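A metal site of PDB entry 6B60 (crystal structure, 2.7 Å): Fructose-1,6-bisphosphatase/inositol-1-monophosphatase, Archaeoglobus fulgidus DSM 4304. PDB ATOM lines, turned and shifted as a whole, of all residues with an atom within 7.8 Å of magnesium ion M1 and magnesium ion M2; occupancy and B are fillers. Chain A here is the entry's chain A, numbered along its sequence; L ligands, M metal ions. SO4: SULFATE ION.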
ATOM      1  N   ASP A  38       7.415  10.712  -7.179  1.00  0.00           N
ATOM      2  CA  ASP A  38       6.524  11.589  -6.460  1.00  0.00           C
ATOM      3  C   ASP A  38       5.071  11.402  -6.879  1.00  0.00           C
ATOM      4  O   ASP A  38       4.134  11.814  -6.173  1.00  0.00           O
ATOM      5  CB  ASP A  38       6.944  13.029  -6.703  1.00  0.00           C
ATOM      6  CG  ASP A  38       6.402  13.570  -7.985  1.00  0.00           C
ATOM      7  OD1 ASP A  38       6.954  13.252  -9.067  1.00  0.00           O
ATOM      8  OD2 ASP A  38       5.418  14.337  -7.885  1.00  0.00           O
ATOM      9  N   THR A  40       3.924  12.431  -9.997  1.00  0.00           N
ATOM     10  CA  THR A  40       3.611  13.326 -11.096  1.00  0.00           C
ATOM     11  C   THR A  40       4.569  13.049 -12.234  1.00  0.00           C
ATOM     12  O   THR A  40       5.660  12.498 -12.027  1.00  0.00           O
ATOM     13  CB  THR A  40       3.665  14.827 -10.724  1.00  0.00           C
ATOM     14  OG1 THR A  40       5.019  15.242 -10.420  1.00  0.00           O
ATOM     15  CG2 THR A  40       2.731  15.101  -9.581  1.00  0.00           C
ATOM     16  N   PRO A  41       4.145  13.403 -13.447  1.00  0.00           N
ATOM     17  CA  PRO A  41       5.025  13.218 -14.598  1.00  0.00           C
ATOM     18  C   PRO A  41       6.413  13.847 -14.369  1.00  0.00           C
ATOM     19  O   PRO A  41       6.538  14.933 -13.778  1.00  0.00           O
ATOM     20  CB  PRO A  41       4.290  13.933 -15.734  1.00  0.00           C
ATOM     21  CG  PRO A  41       2.883  14.181 -15.268  1.00  0.00           C
ATOM     22  CD  PRO A  41       2.872  14.075 -13.781  1.00  0.00           C
ATOM     23  N   THR A  42       7.441  13.138 -14.812  1.00  0.00           N
ATOM     24  CA  THR A  42       8.753  13.722 -15.024  1.00  0.00           C
ATOM     25  C   THR A  42       8.766  14.284 -16.449  1.00  0.00           C
ATOM     26  O   THR A  42       8.460  13.575 -17.391  1.00  0.00           O
ATOM     27  CB  THR A  42       9.848  12.628 -14.902  1.00  0.00           C
ATOM     28  OG1 THR A  42       9.712  11.915 -13.656  1.00  0.00           O
ATOM     29  CG2 THR A  42      11.239  13.222 -15.040  1.00  0.00           C
ATOM     30  N   LYS A  43       9.111  15.550 -16.639  1.00  0.00           N
ATOM     31  CA  LYS A  43       9.354  16.080 -17.977  1.00  0.00           C
ATOM     32  C   LYS A  43      10.843  15.956 -18.330  1.00  0.00           C
ATOM     33  O   LYS A  43      11.680  15.655 -17.460  1.00  0.00           O
ATOM     34  CB  LYS A  43       8.942  17.543 -18.065  1.00  0.00           C
ATOM     35  CG  LYS A  43       7.641  17.838 -17.397  1.00  0.00           C
ATOM     36  CD  LYS A  43       6.628  18.266 -18.399  1.00  0.00           C
ATOM     37  CE  LYS A  43       5.241  18.283 -17.784  1.00  0.00           C
ATOM     38  NZ  LYS A  43       4.182  18.194 -18.829  1.00  0.00           N
ATOM     39  N   ALA A  45      12.891  18.189 -19.086  1.00  0.00           N
ATOM     40  CA  ALA A  45      13.519  19.225 -18.246  1.00  0.00           C
ATOM     41  C   ALA A  45      13.801  18.765 -16.782  1.00  0.00           C
ATOM     42  O   ALA A  45      14.922  18.965 -16.284  1.00  0.00           O
ATOM     43  CB  ALA A  45      12.672  20.499 -18.272  1.00  0.00           C
ATOM     44  N   ASP A  46      12.816  18.159 -16.103  1.00  0.00           N
ATOM     45  CA  ASP A  46      13.049  17.560 -14.782  1.00  0.00           C
ATOM     46  C   ASP A  46      14.147  16.514 -14.816  1.00  0.00           C
ATOM     47  O   ASP A  46      14.995  16.437 -13.917  1.00  0.00           O
ATOM     48  CB  ASP A  46      11.796  16.907 -14.250  1.00  0.00           C
ATOM     49  CG  ASP A  46      10.692  17.897 -14.002  1.00  0.00           C
ATOM     50  OD1 ASP A  46      10.967  19.002 -13.460  1.00  0.00           O
ATOM     51  OD2 ASP A  46       9.541  17.554 -14.373  1.00  0.00           O
ATOM     52  N   ARG A  47      14.139  15.692 -15.861  1.00  0.00           N
ATOM     53  CA  ARG A  47      15.090  14.613 -15.939  1.00  0.00           C
ATOM     54  C   ARG A  47      16.511  15.099 -16.197  1.00  0.00           C
ATOM     55  O   ARG A  47      17.419  14.698 -15.482  1.00  0.00           O
ATOM     56  CB  ARG A  47      14.691  13.582 -16.965  1.00  0.00           C
ATOM     57  CG  ARG A  47      15.372  12.271 -16.734  1.00  0.00           C
ATOM     58  CD  ARG A  47      14.670  11.241 -17.509  1.00  0.00           C
ATOM     59  NE  ARG A  47      13.812  10.402 -16.674  1.00  0.00           N
ATOM     60  CZ  ARG A  47      12.917   9.557 -17.172  1.00  0.00           C
ATOM     61  NH1 ARG A  47      12.738   9.491 -18.485  1.00  0.00           N
ATOM     62  NH2 ARG A  47      12.162   8.807 -16.373  1.00  0.00           N
ATOM     63  N   ALA A  49      17.761  17.949 -15.544  1.00  0.00           N
ATOM     64  CA  ALA A  49      18.098  18.646 -14.294  1.00  0.00           C
ATOM     65  C   ALA A  49      18.461  17.658 -13.195  1.00  0.00           C
ATOM     66  O   ALA A  49      19.550  17.731 -12.641  1.00  0.00           O
ATOM     67  CB  ALA A  49      16.945  19.474 -13.836  1.00  0.00           C
ATOM     68  N   GLU A  50      17.557  16.733 -12.875  1.00  0.00           N
ATOM     69  CA  GLU A  50      17.812  15.800 -11.803  1.00  0.00           C
ATOM     70  C   GLU A  50      19.041  14.958 -12.059  1.00  0.00           C
ATOM     71  O   GLU A  50      19.850  14.757 -11.127  1.00  0.00           O
ATOM     72  CB  GLU A  50      16.642  14.884 -11.579  1.00  0.00           C
ATOM     73  CG  GLU A  50      16.740  14.122 -10.274  1.00  0.00           C
ATOM     74  CD  GLU A  50      15.709  13.020 -10.178  1.00  0.00           C
ATOM     75  OE1 GLU A  50      14.852  13.069  -9.263  1.00  0.00           O
ATOM     76  OE2 GLU A  50      15.752  12.095 -11.028  1.00  0.00           O
ATOM     77  N   THR A  66      14.627  13.254  -3.609  1.00  0.00           N
ATOM     78  CA  THR A  66      14.354  14.077  -4.767  1.00  0.00           C
ATOM     79  C   THR A  66      12.979  13.761  -5.375  1.00  0.00           C
ATOM     80  O   THR A  66      12.354  12.755  -5.032  1.00  0.00           O
ATOM     81  CB  THR A  66      15.466  13.910  -5.800  1.00  0.00           C
ATOM     82  OG1 THR A  66      15.106  14.600  -7.014  1.00  0.00           O
ATOM     83  CG2 THR A  66      15.661  12.468  -6.100  1.00  0.00           C
ATOM     84  N   GLU A  67      12.513  14.635  -6.259  1.00  0.00           N
ATOM     85  CA  GLU A  67      11.142  14.544  -6.710  1.00  0.00           C
ATOM     86  C   GLU A  67      10.901  13.483  -7.770  1.00  0.00           C
ATOM     87  O   GLU A  67       9.854  12.868  -7.824  1.00  0.00           O
ATOM     88  CB  GLU A  67      10.696  15.888  -7.247  1.00  0.00           C
ATOM     89  CG  GLU A  67       9.245  15.888  -7.697  1.00  0.00           C
ATOM     90  CD  GLU A  67       8.897  17.197  -8.353  1.00  0.00           C
ATOM     91  OE1 GLU A  67       7.713  17.450  -8.672  1.00  0.00           O
ATOM     92  OE2 GLU A  67       9.857  17.969  -8.550  1.00  0.00           O
ATOM     93  N   GLU A  68      11.862  13.270  -8.661  1.00  0.00           N
ATOM     94  CA  GLU A  68      11.596  12.353  -9.752  1.00  0.00           C
ATOM     95  C   GLU A  68      12.047  10.946  -9.352  1.00  0.00           C
ATOM     96  O   GLU A  68      11.330   9.972  -9.581  1.00  0.00           O
ATOM     97  CB  GLU A  68      12.235  12.839 -11.064  1.00  0.00           C
ATOM     98  CG  GLU A  68      12.146  14.370 -11.303  1.00  0.00           C
ATOM     99  CD  GLU A  68      10.716  14.922 -11.296  1.00  0.00           C
ATOM    100  OE1 GLU A  68       9.742  14.133 -11.433  1.00  0.00           O
ATOM    101  OE2 GLU A  68      10.582  16.166 -11.147  1.00  0.00           O
ATOM    102  N   LEU A  81      16.017  17.720  -2.392  1.00  0.00           N
ATOM    103  CA  LEU A  81      16.319  18.246  -3.690  1.00  0.00           C
ATOM    104  C   LEU A  81      15.056  18.406  -4.531  1.00  0.00           C
ATOM    105  O   LEU A  81      14.362  17.445  -4.827  1.00  0.00           O
ATOM    106  CB  LEU A  81      17.305  17.310  -4.399  1.00  0.00           C
ATOM    107  CG  LEU A  81      17.597  17.556  -5.878  1.00  0.00           C
ATOM    108  CD1 LEU A  81      18.514  18.769  -6.072  1.00  0.00           C
ATOM    109  CD2 LEU A  81      18.217  16.309  -6.465  1.00  0.00           C
ATOM    110  N   ASP A  82      14.733  19.633  -4.896  1.00  0.00           N
ATOM    111  CA  ASP A  82      13.851  19.807  -6.030  1.00  0.00           C
ATOM    112  C   ASP A  82      14.766  20.108  -7.227  1.00  0.00           C
ATOM    113  O   ASP A  82      15.383  21.171  -7.290  1.00  0.00           O
ATOM    114  CB  ASP A  82      12.801  20.908  -5.812  1.00  0.00           C
ATOM    115  CG  ASP A  82      11.717  20.864  -6.876  1.00  0.00           C
ATOM    116  OD1 ASP A  82      12.034  20.270  -7.924  1.00  0.00           O
ATOM    117  OD2 ASP A  82      10.592  21.393  -6.679  1.00  0.00           O
ATOM    118  N   PRO A  83      14.899  19.147  -8.154  1.00  0.00           N
ATOM    119  CA  PRO A  83      15.942  19.371  -9.156  1.00  0.00           C
ATOM    120  C   PRO A  83      15.517  20.465 -10.120  1.00  0.00           C
ATOM    121  O   PRO A  83      16.369  21.012 -10.820  1.00  0.00           O
ATOM    122  CB  PRO A  83      16.095  17.997  -9.794  1.00  0.00           C
ATOM    123  CG  PRO A  83      14.743  17.374  -9.641  1.00  0.00           C
ATOM    124  CD  PRO A  83      14.149  17.899  -8.396  1.00  0.00           C
ATOM    125  N   LEU A  84      14.235  20.819 -10.125  1.00  0.00           N
ATOM    126  CA  LEU A  84      13.703  21.918 -10.923  1.00  0.00           C
ATOM    127  C   LEU A  84      12.342  22.302 -10.387  1.00  0.00           C
ATOM    128  O   LEU A  84      11.389  21.551 -10.519  1.00  0.00           O
ATOM    129  CB  LEU A  84      13.574  21.521 -12.399  1.00  0.00           C
ATOM    130  CG  LEU A  84      12.813  22.485 -13.317  1.00  0.00           C
ATOM    131  CD1 LEU A  84      13.596  23.748 -13.587  1.00  0.00           C
ATOM    132  CD2 LEU A  84      12.468  21.811 -14.641  1.00  0.00           C
ATOM    133  N   ASP A  85      12.251  23.472  -9.771  1.00  0.00           N
ATOM    134  CA  ASP A  85      11.015  23.930  -9.158  1.00  0.00           C
ATOM    135  C   ASP A  85      10.459  25.014 -10.062  1.00  0.00           C
ATOM    136  O   ASP A  85      11.172  25.963 -10.418  1.00  0.00           O
ATOM    137  CB  ASP A  85      11.288  24.469  -7.744  1.00  0.00           C
ATOM    138  CG  ASP A  85       9.999  24.781  -6.979  1.00  0.00           C
ATOM    139  OD1 ASP A  85       9.289  23.851  -6.535  1.00  0.00           O
ATOM    140  OD2 ASP A  85       9.703  25.974  -6.806  1.00  0.00           O
ATOM    141  N   GLY A  86       9.198  24.877 -10.442  1.00  0.00           N
ATOM    142  CA  GLY A  86       8.587  25.751 -11.441  1.00  0.00           C
ATOM    143  C   GLY A  86       8.733  25.148 -12.825  1.00  0.00           C
ATOM    144  O   GLY A  86       8.901  25.856 -13.806  1.00  0.00           O
ATOM    145  N   THR A  87       8.651  23.817 -12.917  1.00  0.00           N
ATOM    146  CA  THR A  87       8.821  23.141 -14.190  1.00  0.00           C
ATOM    147  C   THR A  87       7.878  23.726 -15.232  1.00  0.00           C
ATOM    148  O   THR A  87       8.252  24.003 -16.378  1.00  0.00           O
ATOM    149  CB  THR A  87       8.530  21.657 -14.060  1.00  0.00           C
ATOM    150  OG1 THR A  87       9.474  21.062 -13.162  1.00  0.00           O
ATOM    151  CG2 THR A  87       8.662  20.989 -15.398  1.00  0.00           C
ATOM    152  N   PHE A  88       6.635  23.928 -14.844  1.00  0.00           N
ATOM    153  CA  PHE A  88       5.676  24.486 -15.774  1.00  0.00           C
ATOM    154  C   PHE A  88       6.229  25.742 -16.421  1.00  0.00           C
ATOM    155  O   PHE A  88       6.190  25.875 -17.629  1.00  0.00           O
ATOM    156  CB  PHE A  88       4.348  24.784 -15.097  1.00  0.00           C
ATOM    157  CG  PHE A  88       3.279  25.129 -16.062  1.00  0.00           C
ATOM    158  CD1 PHE A  88       2.719  24.158 -16.858  1.00  0.00           C
ATOM    159  CD2 PHE A  88       2.839  26.423 -16.181  1.00  0.00           C
ATOM    160  CE1 PHE A  88       1.719  24.470 -17.767  1.00  0.00           C
ATOM    161  CE2 PHE A  88       1.854  26.750 -17.094  1.00  0.00           C
ATOM    162  CZ  PHE A  88       1.294  25.779 -17.890  1.00  0.00           C
ATOM    163  N   SER A  98      13.648  27.350 -10.642  1.00  0.00           N
ATOM    164  CA  SER A  98      14.936  27.150  -9.999  1.00  0.00           C
ATOM    165  C   SER A  98      15.163  25.799  -9.353  1.00  0.00           C
ATOM    166  O   SER A  98      14.258  25.005  -9.203  1.00  0.00           O
ATOM    167  CB  SER A  98      15.223  28.283  -8.978  1.00  0.00           C
ATOM    168  OG  SER A  98      14.115  28.593  -8.149  1.00  0.00           O
ATOM    169  N   SER A 100      16.681  23.705  -5.994  1.00  0.00           N
ATOM    170  CA  SER A 100      16.433  23.948  -4.602  1.00  0.00           C
ATOM    171  C   SER A 100      16.971  22.805  -3.754  1.00  0.00           C
ATOM    172  O   SER A 100      16.490  21.690  -3.803  1.00  0.00           O
ATOM    173  CB  SER A 100      14.937  24.089  -4.358  1.00  0.00           C
ATOM    174  OG  SER A 100      14.645  23.883  -2.979  1.00  0.00           O
ATOM    175  N   ARG A 197       5.533  19.499  -1.113  1.00  0.00           N
ATOM    176  CA  ARG A 197       6.336  18.347  -0.732  1.00  0.00           C
ATOM    177  C   ARG A 197       7.658  18.846  -0.180  1.00  0.00           C
ATOM    178  O   ARG A 197       8.055  19.971  -0.479  1.00  0.00           O
ATOM    179  CB  ARG A 197       6.489  17.431  -1.935  1.00  0.00           C
ATOM    180  CG  ARG A 197       5.116  17.054  -2.480  1.00  0.00           C
ATOM    181  CD  ARG A 197       5.143  16.654  -3.918  1.00  0.00           C
ATOM    182  NE  ARG A 197       5.551  17.780  -4.748  1.00  0.00           N
ATOM    183  CZ  ARG A 197       5.797  17.697  -6.064  1.00  0.00           C
ATOM    184  NH1 ARG A 197       5.672  16.519  -6.672  1.00  0.00           N
ATOM    185  NH2 ARG A 197       6.160  18.786  -6.752  1.00  0.00           N
ATOM    186  N   TYR A 199      10.984  18.617  -0.566  1.00  0.00           N
ATOM    187  CA  TYR A 199      11.912  19.265  -1.485  1.00  0.00           C
ATOM    188  C   TYR A 199      11.372  20.518  -2.202  1.00  0.00           C
ATOM    189  O   TYR A 199      12.148  21.195  -2.877  1.00  0.00           O
ATOM    190  CB  TYR A 199      12.366  18.270  -2.538  1.00  0.00           C
ATOM    191  CG  TYR A 199      11.217  17.462  -3.042  1.00  0.00           C
ATOM    192  CD1 TYR A 199      11.026  16.176  -2.577  1.00  0.00           C
ATOM    193  CD2 TYR A 199      10.291  17.985  -3.953  1.00  0.00           C
ATOM    194  CE1 TYR A 199       9.961  15.412  -3.006  1.00  0.00           C
ATOM    195  CE2 TYR A 199       9.212  17.223  -4.377  1.00  0.00           C
ATOM    196  CZ  TYR A 199       9.071  15.919  -3.896  1.00  0.00           C
ATOM    197  OH  TYR A 199       8.048  15.090  -4.289  1.00  0.00           O
ATOM    198  N   ASP A 200      10.083  20.814  -2.079  1.00  0.00           N
ATOM    199  CA  ASP A 200       9.549  22.119  -2.556  1.00  0.00           C
ATOM    200  C   ASP A 200       9.837  23.252  -1.535  1.00  0.00           C
ATOM    201  O   ASP A 200      10.188  24.369  -1.922  1.00  0.00           O
ATOM    202  CB  ASP A 200       8.032  22.105  -2.781  1.00  0.00           C
ATOM    203  CG  ASP A 200       7.603  21.319  -3.986  1.00  0.00           C
ATOM    204  OD1 ASP A 200       8.189  21.480  -5.071  1.00  0.00           O
ATOM    205  OD2 ASP A 200       6.643  20.525  -3.826  1.00  0.00           O
HETATM  206  S   SO4 L   1       7.714  21.031  -9.766  1.00  0.00           S
HETATM  207  O1  SO4 L   1       7.640  22.335 -10.434  1.00  0.00           O
HETATM  208  O2  SO4 L   1       8.099  21.265  -8.345  1.00  0.00           O
HETATM  209  O3  SO4 L   1       8.599  20.171 -10.594  1.00  0.00           O
HETATM  210  O4  SO4 L   1       6.406  20.352  -9.772  1.00  0.00           O
HETATM  211 MG    MG M   1      10.064  20.245  -8.944  1.00  0.00          MG
HETATM  212 MG    MG M   2      11.422  18.965 -10.230  1.00  0.00          MG
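The side-chain carboxylate of Asp 46 sits at hydrogen-bond distance from the side-chain hydroxyl of Thr 87, at 2.6 Å.
The backbone carbonyl oxygen (O) of Leu 84 lies close to the side-chain hydroxyl (OG1) of Thr 87 (3.3 Å).
N of Glu 68 lies within hydrogen-bond range of OE1 of Glu 50 (3.1 Å).
The side-chain carboxylate (OE1) of Glu 67 lies within salt-bridge range of the guanidinium group (NH2) of Arg 197 (2.8 Å).
O of Glu 67 lies close to N of Asp 38 (3.3 Å).
The backbone NH (N) of Lys 43 sits at hydrogen-bond distance from the side-chain carboxylate (OD2) of Asp 46 (3.1 Å).
O of Ser 100 is in hydrogen-bond range of N of Asp 82, at 2.9 Å.
The side-chain hydroxyl (OG1) of Thr 42 is in hydrogen-bond range of the side-chain carboxylate (OE1) of Glu 68 (3.1 Å).
Merely in contact with magnesium ion M1: Asp 85 (3.8 Å).
Within 4 Å of magnesium ion M1: Glu 67, Asp 82, Leu 84 and Asp 85.
Residues that only touch magnesium ion M2: Asp 46 (3.3 Å), Glu 68 (3.1 Å) and Pro 83 (3.5 Å).
Magnesium ion M1 is bound by O3 of the ligand, OD1 of Asp 82, O2 of the ligand, OE2 of Glu 67, O of Leu 84 and OD2 of Asp 82.
OE2 of Glu 67 is bound to magnesium ion M2 (2.5 Å).
Magnesium ion M2 has one donor atom within binding distance.
Slightly farther from magnesium ion M2 lies the backbone carbonyl oxygen (O) of Leu 84 (2.6 Å).
Slightly farther from magnesium ion M2 lies the side-chain carboxylate (OD1) of Asp 82 (2.7 Å).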
